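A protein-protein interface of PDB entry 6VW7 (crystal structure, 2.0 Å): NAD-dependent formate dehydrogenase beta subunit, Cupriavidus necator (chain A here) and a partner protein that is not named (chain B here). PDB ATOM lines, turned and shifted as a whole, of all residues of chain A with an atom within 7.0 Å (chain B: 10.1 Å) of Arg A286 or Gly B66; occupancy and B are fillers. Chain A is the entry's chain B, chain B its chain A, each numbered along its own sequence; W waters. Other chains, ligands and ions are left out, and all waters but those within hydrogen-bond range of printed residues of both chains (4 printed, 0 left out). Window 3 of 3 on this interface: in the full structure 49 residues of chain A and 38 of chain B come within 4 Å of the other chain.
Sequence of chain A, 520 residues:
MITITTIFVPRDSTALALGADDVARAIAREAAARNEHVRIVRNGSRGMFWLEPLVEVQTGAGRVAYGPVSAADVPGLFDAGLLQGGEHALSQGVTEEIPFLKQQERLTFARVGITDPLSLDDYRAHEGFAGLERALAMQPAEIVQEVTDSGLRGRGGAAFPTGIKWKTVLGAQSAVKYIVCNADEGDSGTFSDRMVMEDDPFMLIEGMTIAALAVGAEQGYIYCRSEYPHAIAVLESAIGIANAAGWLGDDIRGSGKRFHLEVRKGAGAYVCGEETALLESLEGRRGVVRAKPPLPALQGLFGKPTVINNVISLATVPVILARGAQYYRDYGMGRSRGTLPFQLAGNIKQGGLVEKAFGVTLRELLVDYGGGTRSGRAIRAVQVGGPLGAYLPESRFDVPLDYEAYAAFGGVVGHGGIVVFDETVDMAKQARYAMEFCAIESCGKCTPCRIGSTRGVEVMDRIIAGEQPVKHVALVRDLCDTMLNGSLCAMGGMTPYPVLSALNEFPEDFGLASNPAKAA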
ATOM      1  N   CYS A 272       7.366 -32.286  20.836  1.00  0.00           N
ATOM      2  CA  CYS A 272       6.108 -31.591  21.080  1.00  0.00           C
ATOM      3  C   CYS A 272       5.030 -31.911  20.045  1.00  0.00           C
ATOM      4  O   CYS A 272       3.934 -31.358  20.152  1.00  0.00           O
ATOM      5  CB  CYS A 272       6.333 -30.068  21.164  1.00  0.00           C
ATOM      6  SG  CYS A 272       7.138 -29.598  22.737  1.00  0.00           S
ATOM      7  N   THR A 276       0.648 -35.083  24.632  1.00  0.00           N
ATOM      8  CA  THR A 276       0.783 -34.553  25.990  1.00  0.00           C
ATOM      9  C   THR A 276       2.002 -33.656  26.158  1.00  0.00           C
ATOM     10  O   THR A 276       1.968 -32.747  26.997  1.00  0.00           O
ATOM     11  CB  THR A 276       0.804 -35.672  27.046  1.00  0.00           C
ATOM     12  OG1 THR A 276       1.914 -36.562  26.843  1.00  0.00           O
ATOM     13  CG2 THR A 276      -0.486 -36.427  27.019  1.00  0.00           C
ATOM     14  N   ALA A 277       3.089 -33.900  25.419  1.00  0.00           N
ATOM     15  CA  ALA A 277       4.197 -32.946  25.460  1.00  0.00           C
ATOM     16  C   ALA A 277       3.778 -31.619  24.840  1.00  0.00           C
ATOM     17  O   ALA A 277       4.186 -30.545  25.307  1.00  0.00           O
ATOM     18  CB  ALA A 277       5.430 -33.499  24.742  1.00  0.00           C
ATOM     19  N   LEU A 279       0.716 -30.419  25.090  1.00  0.00           N
ATOM     20  CA  LEU A 279      -0.048 -29.729  26.124  1.00  0.00           C
ATOM     21  C   LEU A 279       0.870 -29.074  27.152  1.00  0.00           C
ATOM     22  O   LEU A 279       0.642 -27.920  27.543  1.00  0.00           O
ATOM     23  CB  LEU A 279      -1.022 -30.685  26.815  1.00  0.00           C
ATOM     24  CG  LEU A 279      -2.096 -31.340  25.936  1.00  0.00           C
ATOM     25  CD1 LEU A 279      -2.983 -32.248  26.793  1.00  0.00           C
ATOM     26  CD2 LEU A 279      -2.936 -30.298  25.226  1.00  0.00           C
ATOM     27  N   GLU A 280       1.914 -29.783  27.593  1.00  0.00           N
ATOM     28  CA  GLU A 280       2.873 -29.179  28.519  1.00  0.00           C
ATOM     29  C   GLU A 280       3.448 -27.875  27.958  1.00  0.00           C
ATOM     30  O   GLU A 280       3.563 -26.870  28.678  1.00  0.00           O
ATOM     31  CB  GLU A 280       3.990 -30.172  28.830  1.00  0.00           C
ATOM     32  CG  GLU A 280       3.552 -31.342  29.755  1.00  0.00           C
ATOM     33  CD  GLU A 280       3.159 -30.840  31.137  1.00  0.00           C
ATOM     34  OE1 GLU A 280       1.952 -30.812  31.446  1.00  0.00           O
ATOM     35  OE2 GLU A 280       4.062 -30.441  31.901  1.00  0.00           O
ATOM     36  N   SER A 281       3.799 -27.880  26.671  1.00  0.00           N
ATOM     37  CA  SER A 281       4.347 -26.701  26.009  1.00  0.00           C
ATOM     38  C   SER A 281       3.331 -25.565  25.975  1.00  0.00           C
ATOM     39  O   SER A 281       3.650 -24.422  26.323  1.00  0.00           O
ATOM     40  CB  SER A 281       4.788 -27.075  24.589  1.00  0.00           C
ATOM     41  OG  SER A 281       5.701 -26.132  24.056  1.00  0.00           O
ATOM     42  N   GLY A 284       3.257 -23.815  29.018  1.00  0.00           N
ATOM     43  CA  GLY A 284       4.461 -23.071  29.320  1.00  0.00           C
ATOM     44  C   GLY A 284       5.580 -23.865  29.943  1.00  0.00           C
ATOM     45  O   GLY A 284       6.499 -23.268  30.514  1.00  0.00           O
ATOM     46  N   ARG A 285       5.542 -25.190  29.865  1.00  0.00           N
ATOM     47  CA  ARG A 285       6.538 -26.016  30.529  1.00  0.00           C
ATOM     48  C   ARG A 285       7.371 -26.770  29.499  1.00  0.00           C
ATOM     49  O   ARG A 285       7.077 -26.771  28.303  1.00  0.00           O
ATOM     50  CB  ARG A 285       5.873 -26.984  31.523  1.00  0.00           C
ATOM     51  CG  ARG A 285       5.298 -26.284  32.764  1.00  0.00           C
ATOM     52  CD  ARG A 285       4.777 -27.276  33.821  1.00  0.00           C
ATOM     53  NE  ARG A 285       3.619 -28.011  33.318  1.00  0.00           N
ATOM     54  CZ  ARG A 285       2.366 -27.577  33.415  1.00  0.00           C
ATOM     55  NH1 ARG A 285       2.107 -26.421  34.012  1.00  0.00           N
ATOM     56  NH2 ARG A 285       1.373 -28.290  32.901  1.00  0.00           N
ATOM     57  N   ARG A 286       8.440 -27.405  29.972  1.00  0.00           N
ATOM     58  CA  ARG A 286       9.232 -28.256  29.093  1.00  0.00           C
ATOM     59  C   ARG A 286       8.335 -29.315  28.450  1.00  0.00           C
ATOM     60  O   ARG A 286       7.357 -29.765  29.041  1.00  0.00           O
ATOM     61  CB  ARG A 286      10.373 -28.902  29.870  1.00  0.00           C
ATOM     62  CG  ARG A 286      11.305 -27.875  30.512  1.00  0.00           C
ATOM     63  CD  ARG A 286      12.059 -28.445  31.703  1.00  0.00           C
ATOM     64  NE  ARG A 286      13.097 -29.368  31.282  1.00  0.00           N
ATOM     65  CZ  ARG A 286      13.119 -30.661  31.596  1.00  0.00           C
ATOM     66  NH1 ARG A 286      14.112 -31.427  31.156  1.00  0.00           N
ATOM     67  NH2 ARG A 286      12.162 -31.189  32.361  1.00  0.00           N
ATOM     68  N   GLY A 287       8.640 -29.655  27.198  1.00  0.00           N
ATOM     69  CA  GLY A 287       7.813 -30.581  26.446  1.00  0.00           C
ATOM     70  C   GLY A 287       8.045 -32.031  26.829  1.00  0.00           C
ATOM     71  O   GLY A 287       8.477 -32.838  26.004  1.00  0.00           O
ATOM     72  N   VAL A 288       7.766 -32.378  28.081  1.00  0.00           N
ATOM     73  CA  VAL A 288       7.993 -33.731  28.590  1.00  0.00           C
ATOM     74  C   VAL A 288       6.682 -34.511  28.521  1.00  0.00           C
ATOM     75  O   VAL A 288       5.647 -34.052  29.018  1.00  0.00           O
ATOM     76  CB  VAL A 288       8.553 -33.687  30.022  1.00  0.00           C
ATOM     77  CG1 VAL A 288       8.720 -35.115  30.601  1.00  0.00           C
ATOM     78  CG2 VAL A 288       9.879 -32.918  30.044  1.00  0.00           C
ATOM     79  N   VAL A 289       6.719 -35.690  27.892  1.00  0.00           N
ATOM     80  CA  VAL A 289       5.512 -36.496  27.745  1.00  0.00           C
ATOM     81  C   VAL A 289       4.880 -36.775  29.108  1.00  0.00           C
ATOM     82  O   VAL A 289       5.576 -37.056  30.088  1.00  0.00           O
ATOM     83  CB  VAL A 289       5.875 -37.813  27.035  1.00  0.00           C
ATOM     84  CG1 VAL A 289       4.686 -38.766  27.012  1.00  0.00           C
ATOM     85  CG2 VAL A 289       6.378 -37.542  25.619  1.00  0.00           C
ATOM     86  N   CYS A 443      12.893 -36.163  24.989  1.00  0.00           N
ATOM     87  CA  CYS A 443      12.461 -35.299  26.083  1.00  0.00           C
ATOM     88  C   CYS A 443      13.168 -35.649  27.393  1.00  0.00           C
ATOM     89  O   CYS A 443      13.156 -34.839  28.329  1.00  0.00           O
ATOM     90  CB  CYS A 443      10.929 -35.333  26.217  1.00  0.00           C
ATOM     91  SG  CYS A 443      10.230 -36.547  27.357  1.00  0.00           S
ATOM     92  N   GLY A 444      13.784 -36.830  27.485  1.00  0.00           N
ATOM     93  CA  GLY A 444      14.642 -37.159  28.605  1.00  0.00           C
ATOM     94  C   GLY A 444      14.022 -38.026  29.682  1.00  0.00           C
ATOM     95  O   GLY A 444      14.724 -38.411  30.624  1.00  0.00           O
ATOM     96  N   LEU B  31       4.480 -18.455  29.172  1.00  0.00           N
ATOM     97  CA  LEU B  31       5.945 -18.442  29.172  1.00  0.00           C
ATOM     98  C   LEU B  31       6.519 -18.490  27.755  1.00  0.00           C
ATOM     99  O   LEU B  31       7.392 -17.681  27.416  1.00  0.00           O
ATOM    100  CB  LEU B  31       6.507 -19.579  30.024  1.00  0.00           C
ATOM    101  CG  LEU B  31       8.034 -19.595  30.136  1.00  0.00           C
ATOM    102  CD1 LEU B  31       8.569 -18.198  30.434  1.00  0.00           C
ATOM    103  CD2 LEU B  31       8.491 -20.573  31.223  1.00  0.00           C
ATOM    104  N   LEU B  32       6.084 -19.456  26.922  1.00  0.00           N
ATOM    105  CA  LEU B  32       6.623 -19.531  25.561  1.00  0.00           C
ATOM    106  C   LEU B  32       6.292 -18.302  24.713  1.00  0.00           C
ATOM    107  O   LEU B  32       7.179 -17.856  23.966  1.00  0.00           O
ATOM    108  CB  LEU B  32       6.161 -20.815  24.849  1.00  0.00           C
ATOM    109  CG  LEU B  32       7.184 -21.953  24.909  1.00  0.00           C
ATOM    110  CD1 LEU B  32       7.244 -22.495  26.315  1.00  0.00           C
ATOM    111  CD2 LEU B  32       6.891 -23.106  23.906  1.00  0.00           C
ATOM    112  N   LEU B  35       8.796 -15.758  25.868  1.00  0.00           N
ATOM    113  CA  LEU B  35      10.156 -16.030  25.415  1.00  0.00           C
ATOM    114  C   LEU B  35      10.307 -15.727  23.929  1.00  0.00           C
ATOM    115  O   LEU B  35      11.336 -15.192  23.503  1.00  0.00           O
ATOM    116  CB  LEU B  35      10.533 -17.489  25.712  1.00  0.00           C
ATOM    117  CG  LEU B  35      10.674 -17.866  27.194  1.00  0.00           C
ATOM    118  CD1 LEU B  35      10.932 -19.395  27.382  1.00  0.00           C
ATOM    119  CD2 LEU B  35      11.774 -17.068  27.843  1.00  0.00           C
ATOM    120  N   ILE B  45      17.311 -14.340  24.722  1.00  0.00           N
ATOM    121  CA  ILE B  45      16.713 -14.144  26.037  1.00  0.00           C
ATOM    122  C   ILE B  45      17.853 -13.932  27.027  1.00  0.00           C
ATOM    123  O   ILE B  45      18.551 -14.897  27.375  1.00  0.00           O
ATOM    124  CB  ILE B  45      15.828 -15.328  26.448  1.00  0.00           C
ATOM    125  CG1 ILE B  45      14.655 -15.469  25.471  1.00  0.00           C
ATOM    126  CG2 ILE B  45      15.333 -15.160  27.883  1.00  0.00           C
ATOM    127  CD1 ILE B  45      14.676 -16.753  24.765  1.00  0.00           C
ATOM    128  N   ASP B  47      19.974 -13.576  30.439  1.00  0.00           N
ATOM    129  CA  ASP B  47      19.836 -14.161  31.771  1.00  0.00           C
ATOM    130  C   ASP B  47      19.111 -13.211  32.713  1.00  0.00           C
ATOM    131  O   ASP B  47      18.348 -13.646  33.585  1.00  0.00           O
ATOM    132  CB  ASP B  47      21.214 -14.513  32.337  1.00  0.00           C
ATOM    133  CG  ASP B  47      21.751 -15.850  31.819  1.00  0.00           C
ATOM    134  OD1 ASP B  47      20.993 -16.634  31.198  1.00  0.00           O
ATOM    135  OD2 ASP B  47      22.959 -16.097  32.029  1.00  0.00           O
ATOM    136  N   VAL B  50      15.259 -13.526  33.264  1.00  0.00           N
ATOM    137  CA  VAL B  50      14.623 -14.659  33.942  1.00  0.00           C
ATOM    138  C   VAL B  50      13.952 -14.247  35.250  1.00  0.00           C
ATOM    139  O   VAL B  50      12.782 -14.608  35.455  1.00  0.00           O
ATOM    140  CB  VAL B  50      15.628 -15.807  34.111  1.00  0.00           C
ATOM    141  CG1 VAL B  50      15.018 -16.942  34.950  1.00  0.00           C
ATOM    142  CG2 VAL B  50      16.055 -16.317  32.725  1.00  0.00           C
ATOM    143  N   ILE B  53      10.625 -12.537  34.368  1.00  0.00           N
ATOM    144  CA  ILE B  53       9.623 -13.497  33.918  1.00  0.00           C
ATOM    145  C   ILE B  53       9.108 -14.311  35.100  1.00  0.00           C
ATOM    146  O   ILE B  53       7.896 -14.417  35.318  1.00  0.00           O
ATOM    147  CB  ILE B  53      10.218 -14.407  32.830  1.00  0.00           C
ATOM    148  CG1 ILE B  53      10.631 -13.582  31.609  1.00  0.00           C
ATOM    149  CG2 ILE B  53       9.260 -15.562  32.487  1.00  0.00           C
ATOM    150  CD1 ILE B  53      11.680 -14.266  30.745  1.00  0.00           C
ATOM    151  N   ALA B  54      10.030 -14.839  35.912  1.00  0.00           N
ATOM    152  CA  ALA B  54       9.655 -15.712  37.023  1.00  0.00           C
ATOM    153  C   ALA B  54       8.671 -15.027  37.958  1.00  0.00           C
ATOM    154  O   ALA B  54       7.626 -15.594  38.300  1.00  0.00           O
ATOM    155  CB  ALA B  54      10.903 -16.157  37.787  1.00  0.00           C
ATOM    156  N   LEU B  59       6.496 -18.236  38.853  1.00  0.00           N
ATOM    157  CA  LEU B  59       7.297 -19.427  38.598  1.00  0.00           C
ATOM    158  C   LEU B  59       8.652 -19.247  39.266  1.00  0.00           C
ATOM    159  O   LEU B  59       9.060 -18.127  39.580  1.00  0.00           O
ATOM    160  CB  LEU B  59       7.487 -19.669  37.093  1.00  0.00           C
ATOM    161  CG  LEU B  59       6.249 -19.927  36.234  1.00  0.00           C
ATOM    162  CD1 LEU B  59       6.634 -19.993  34.780  1.00  0.00           C
ATOM    163  CD2 LEU B  59       5.583 -21.235  36.658  1.00  0.00           C
ATOM    164  N   SER B  60       9.368 -20.347  39.475  1.00  0.00           N
ATOM    165  CA  SER B  60      10.715 -20.187  39.999  1.00  0.00           C
ATOM    166  C   SER B  60      11.673 -19.826  38.870  1.00  0.00           C
ATOM    167  O   SER B  60      11.414 -20.085  37.691  1.00  0.00           O
ATOM    168  CB  SER B  60      11.197 -21.466  40.679  1.00  0.00           C
ATOM    169  OG  SER B  60      11.566 -22.400  39.681  1.00  0.00           O
ATOM    170  N   ARG B  61      12.803 -19.232  39.244  1.00  0.00           N
ATOM    171  CA  ARG B  61      13.817 -18.905  38.246  1.00  0.00           C
ATOM    172  C   ARG B  61      14.353 -20.167  37.581  1.00  0.00           C
ATOM    173  O   ARG B  61      14.605 -20.180  36.370  1.00  0.00           O
ATOM    174  CB  ARG B  61      14.956 -18.104  38.880  1.00  0.00           C
ATOM    175  CG  ARG B  61      14.594 -16.674  39.320  1.00  0.00           C
ATOM    176  CD  ARG B  61      13.941 -16.646  40.709  1.00  0.00           C
ATOM    177  NE  ARG B  61      14.293 -17.826  41.500  1.00  0.00           N
ATOM    178  CZ  ARG B  61      13.597 -18.284  42.539  1.00  0.00           C
ATOM    179  NH1 ARG B  61      12.495 -17.672  42.942  1.00  0.00           N
ATOM    180  NH2 ARG B  61      14.010 -19.367  43.176  1.00  0.00           N
ATOM    181  N   ALA B  62      14.535 -21.243  38.353  1.00  0.00           N
ATOM    182  CA  ALA B  62      15.040 -22.488  37.770  1.00  0.00           C
ATOM    183  C   ALA B  62      14.059 -23.058  36.755  1.00  0.00           C
ATOM    184  O   ALA B  62      14.459 -23.560  35.696  1.00  0.00           O
ATOM    185  CB  ALA B  62      15.319 -23.513  38.872  1.00  0.00           C
ATOM    186  N   GLU B  63      12.765 -22.960  37.049  1.00  0.00           N
ATOM    187  CA  GLU B  63      11.748 -23.415  36.111  1.00  0.00           C
ATOM    188  C   GLU B  63      11.869 -22.682  34.776  1.00  0.00           C
ATOM    189  O   GLU B  63      11.901 -23.305  33.706  1.00  0.00           O
ATOM    190  CB  GLU B  63      10.369 -23.215  36.739  1.00  0.00           C
ATOM    191  CG  GLU B  63       9.208 -23.251  35.775  1.00  0.00           C
ATOM    192  CD  GLU B  63       8.892 -24.655  35.308  1.00  0.00           C
ATOM    193  OE1 GLU B  63       9.377 -25.605  35.944  1.00  0.00           O
ATOM    194  OE2 GLU B  63       8.161 -24.809  34.304  1.00  0.00           O
ATOM    195  N   VAL B  64      11.950 -21.346  34.825  1.00  0.00           N
ATOM    196  CA  VAL B  64      12.057 -20.556  33.602  1.00  0.00           C
ATOM    197  C   VAL B  64      13.335 -20.913  32.848  1.00  0.00           C
ATOM    198  O   VAL B  64      13.314 -21.142  31.633  1.00  0.00           O
ATOM    199  CB  VAL B  64      11.998 -19.049  33.936  1.00  0.00           C
ATOM    200  CG1 VAL B  64      12.189 -18.214  32.678  1.00  0.00           C
ATOM    201  CG2 VAL B  64      10.670 -18.707  34.605  1.00  0.00           C
ATOM    202  N   HIS B  65      14.470 -20.963  33.559  1.00  0.00           N
ATOM    203  CA  HIS B  65      15.719 -21.319  32.898  1.00  0.00           C
ATOM    204  C   HIS B  65      15.644 -22.717  32.283  1.00  0.00           C
ATOM    205  O   HIS B  65      16.195 -22.955  31.198  1.00  0.00           O
ATOM    206  CB  HIS B  65      16.884 -21.208  33.884  1.00  0.00           C
ATOM    207  CG  HIS B  65      18.207 -21.580  33.293  1.00  0.00           C
ATOM    208  ND1 HIS B  65      18.819 -22.789  33.544  1.00  0.00           N
ATOM    209  CD2 HIS B  65      19.026 -20.909  32.449  1.00  0.00           C
ATOM    210  CE1 HIS B  65      19.964 -22.844  32.887  1.00  0.00           C
ATOM    211  NE2 HIS B  65      20.113 -21.717  32.215  1.00  0.00           N
ATOM    212  N   GLY B  66      14.945 -23.645  32.935  1.00  0.00           N
ATOM    213  CA  GLY B  66      14.831 -24.989  32.382  1.00  0.00           C
ATOM    214  C   GLY B  66      14.041 -25.019  31.085  1.00  0.00           C
ATOM    215  O   GLY B  66      14.343 -25.801  30.178  1.00  0.00           O
ATOM    216  N   VAL B  67      13.022 -24.165  30.974  1.00  0.00           N
ATOM    217  CA  VAL B  67      12.281 -24.062  29.719  1.00  0.00           C
ATOM    218  C   VAL B  67      13.172 -23.490  28.621  1.00  0.00           C
ATOM    219  O   VAL B  67      13.241 -24.033  27.511  1.00  0.00           O
ATOM    220  CB  VAL B  67      11.007 -23.221  29.930  1.00  0.00           C
ATOM    221  CG1 VAL B  67      10.354 -22.822  28.582  1.00  0.00           C
ATOM    222  CG2 VAL B  67      10.025 -23.987  30.837  1.00  0.00           C
ATOM    223  N   ILE B  68      13.888 -22.399  28.922  1.00  0.00           N
ATOM    224  CA  ILE B  68      14.780 -21.794  27.936  1.00  0.00           C
ATOM    225  C   ILE B  68      15.790 -22.817  27.441  1.00  0.00           C
ATOM    226  O   ILE B  68      16.056 -22.923  26.235  1.00  0.00           O
ATOM    227  CB  ILE B  68      15.480 -20.557  28.534  1.00  0.00           C
ATOM    228  CG1 ILE B  68      14.467 -19.455  28.847  1.00  0.00           C
ATOM    229  CG2 ILE B  68      16.538 -20.039  27.583  1.00  0.00           C
ATOM    230  CD1 ILE B  68      15.031 -18.345  29.759  1.00  0.00           C
ATOM    231  N   THR B  69      16.351 -23.605  28.365  1.00  0.00           N
ATOM    232  CA  THR B  69      17.355 -24.601  28.016  1.00  0.00           C
ATOM    233  C   THR B  69      16.766 -25.773  27.234  1.00  0.00           C
ATOM    234  O   THR B  69      17.438 -26.334  26.361  1.00  0.00           O
ATOM    235  CB  THR B  69      18.038 -25.093  29.299  1.00  0.00           C
ATOM    236  OG1 THR B  69      18.826 -24.027  29.844  1.00  0.00           O
ATOM    237  CG2 THR B  69      18.931 -26.282  29.029  1.00  0.00           C
ATOM    238  N   PHE B  70      15.518 -26.147  27.517  1.00  0.00           N
ATOM    239  CA  PHE B  70      14.924 -27.319  26.875  1.00  0.00           C
ATOM    240  C   PHE B  70      14.723 -27.103  25.378  1.00  0.00           C
ATOM    241  O   PHE B  70      14.950 -28.014  24.574  1.00  0.00           O
ATOM    242  CB  PHE B  70      13.587 -27.651  27.554  1.00  0.00           C
ATOM    243  CG  PHE B  70      12.890 -28.886  26.991  1.00  0.00           C
ATOM    244  CD1 PHE B  70      13.158 -30.143  27.516  1.00  0.00           C
ATOM    245  CD2 PHE B  70      11.959 -28.775  25.963  1.00  0.00           C
ATOM    246  CE1 PHE B  70      12.525 -31.278  27.006  1.00  0.00           C
ATOM    247  CE2 PHE B  70      11.315 -29.897  25.451  1.00  0.00           C
ATOM    248  CZ  PHE B  70      11.606 -31.163  25.982  1.00  0.00           C
ATOM    249  N   TYR B  71      14.287 -25.915  24.978  1.00  0.00           N
ATOM    250  CA  TYR B  71      13.821 -25.690  23.616  1.00  0.00           C
ATOM    251  C   TYR B  71      14.955 -25.123  22.771  1.00  0.00           C
ATOM    252  O   TYR B  71      15.432 -24.013  23.032  1.00  0.00           O
ATOM    253  CB  TYR B  71      12.608 -24.757  23.610  1.00  0.00           C
ATOM    254  CG  TYR B  71      11.336 -25.377  24.174  1.00  0.00           C
ATOM    255  CD1 TYR B  71      10.546 -26.250  23.415  1.00  0.00           C
ATOM    256  CD2 TYR B  71      10.919 -25.076  25.463  1.00  0.00           C
ATOM    257  CE1 TYR B  71       9.359 -26.815  23.952  1.00  0.00           C
ATOM    258  CE2 TYR B  71       9.757 -25.622  26.002  1.00  0.00           C
ATOM    259  CZ  TYR B  71       8.991 -26.505  25.250  1.00  0.00           C
ATOM    260  OH  TYR B  71       7.846 -27.016  25.806  1.00  0.00           O
ATOM    261  N   HIS B  72      15.343 -25.868  21.731  1.00  0.00           N
ATOM    262  CA  HIS B  72      16.471 -25.497  20.883  1.00  0.00           C
ATOM    263  C   HIS B  72      16.253 -24.178  20.153  1.00  0.00           C
ATOM    264  O   HIS B  72      17.226 -23.537  19.746  1.00  0.00           O
ATOM    265  CB  HIS B  72      16.734 -26.612  19.862  1.00  0.00           C
ATOM    266  CG  HIS B  72      17.138 -27.919  20.478  1.00  0.00           C
ATOM    267  ND1 HIS B  72      16.562 -29.121  20.120  1.00  0.00           N
ATOM    268  CD2 HIS B  72      18.072 -28.215  21.412  1.00  0.00           C
ATOM    269  CE1 HIS B  72      17.116 -30.099  20.817  1.00  0.00           C
ATOM    270  NE2 HIS B  72      18.038 -29.576  21.604  1.00  0.00           N
ATOM    271  N   PHE B  74      15.328 -21.380  21.315  1.00  0.00           N
ATOM    272  CA  PHE B  74      15.660 -20.208  22.133  1.00  0.00           C
ATOM    273  C   PHE B  74      17.165 -20.095  22.327  1.00  0.00           C
ATOM    274  O   PHE B  74      17.834 -21.086  22.623  1.00  0.00           O
ATOM    275  CB  PHE B  74      14.969 -20.291  23.500  1.00  0.00           C
ATOM    276  CG  PHE B  74      13.462 -20.203  23.426  1.00  0.00           C
ATOM    277  CD1 PHE B  74      12.848 -19.218  22.668  1.00  0.00           C
ATOM    278  CD2 PHE B  74      12.666 -21.102  24.119  1.00  0.00           C
ATOM    279  CE1 PHE B  74      11.462 -19.135  22.589  1.00  0.00           C
ATOM    280  CE2 PHE B  74      11.280 -21.027  24.047  1.00  0.00           C
ATOM    281  CZ  PHE B  74      10.675 -20.059  23.283  1.00  0.00           C
ATOM    282  N   GLN B  76      20.336 -17.902  24.351  1.00  0.00           N
ATOM    283  CA  GLN B  76      20.631 -17.069  25.508  1.00  0.00           C
ATOM    284  C   GLN B  76      21.750 -16.070  25.256  1.00  0.00           C
ATOM    285  O   GLN B  76      22.122 -15.337  26.172  1.00  0.00           O
ATOM    286  CB  GLN B  76      20.968 -17.954  26.713  1.00  0.00           C
ATOM    287  CG  GLN B  76      19.761 -18.718  27.214  1.00  0.00           C
ATOM    288  CD  GLN B  76      20.079 -19.686  28.336  1.00  0.00           C
ATOM    289  OE1 GLN B  76      19.739 -19.440  29.497  1.00  0.00           O
ATOM    290  NE2 GLN B  76      20.718 -20.808  27.993  1.00  0.00           N
HETATM  291  O   HOH W   1       6.789 -22.968  33.174  1.00  0.00           O
HETATM  292  O   HOH W   2       8.915 -27.062  32.900  1.00  0.00           O
HETATM  293  O   HOH W   3      15.617 -28.480  30.533  1.00  0.00           O
HETATM  294  O   HOH W   4       3.468 -21.661  26.397  1.00  0.00           O
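The side-chain hydroxyl (OG) of Ser B60 is in hydrogen-bond range of the backbone NH (N) of Glu B63 (2.9 Å).
The side-chain carboxylate of Glu A280 is in salt-bridge range of the guanidinium group of Arg A285, at 2.8 Å.
The backbone NH (N) of Val A289 sits close to the side-chain sulfur (SG) of Cys A443 (3.7 Å).
Among the printed residues, pairs that only touch across the chains: Gly A287 with Phe B70, Ser A281 with Leu B32, Gly A284 with Leu B31, Arg A286 with Tyr B71, Arg A285 with Glu B63, Gly A284 with Val B67, Arg A286 with Gly B66, Arg A286 with Phe B70, Cys A272 with Tyr B71, Cys A443 with Phe B70 and Arg A286 with Val B67.
OG of Ser A281 sits at hydrogen-bond distance from OH of Tyr B71 (2.9 Å).
The side-chain hydroxyl (OH) of Tyr B71 is in hydrogen-bond range of the backbone carbonyl oxygen (O) of Arg A285, 2.6 Å away.
The backbone NH (N) of Gly A287 is in hydrogen-bond range of the side-chain hydroxyl (OH) of Tyr B71 (3.1 Å).
No residue of chain B comes within 4 Å of Glu A280.
Of the printed residues of chain B, Gly A284 touches Leu B31 (3.4 Å) and Val B67 (3.6 Å).
Of the printed residues of chain B, Arg A285 touches Glu B63 (3.6 Å) and Tyr B71 (2.6 Å).
Of chain B, only Gly B66 (3.7 Å), Val B67 (3.9 Å), Phe B70 (3.7 Å) and Tyr B71 (3.5 Å) come within 4 Å of Arg A286.
Of chain B, only Phe B70 and Tyr B71 come within 4 Å of Gly A287.
Printed residues of chain A within 4 Å of Leu B32: Ser A281.
Val B50 touches none of the printed residues of chain A.
Of the printed residues of chain A, Glu B63 touches Arg A285.
Of chain A, only Arg A286 comes within 4 Å of Gly B66.
Thr B69 touches none of the printed residues of chain A.
Printed residues of chain A within 4 Å of Tyr B71: Cys A272, Ser A281, Arg A285, Arg A286 and Gly A287.
Along chain B the printed residues that touch a printed residue of chain A span positions 31 to 71.
Among the printed residues, no Asp or Glu carboxylate lies within 4 Å of a Lys or Arg side-chain nitrogen of the other chain.
Water W1 bridges OE2 of Glu B63 and O of Gly A284.
Water W2 lies within hydrogen-bond range of OE2 of Glu B63 (2.8 Å) and N of Arg A286 (3.0 Å).
Water W4 lies within hydrogen-bond range of O of Ser A281 (2.8 Å), N of Gly A284 (3.4 Å) and N of Leu B32 (3.5 Å).
Water W3 bridges NE of Arg A286 (2.8 Å) and O of Gly B66 (3.0 Å).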
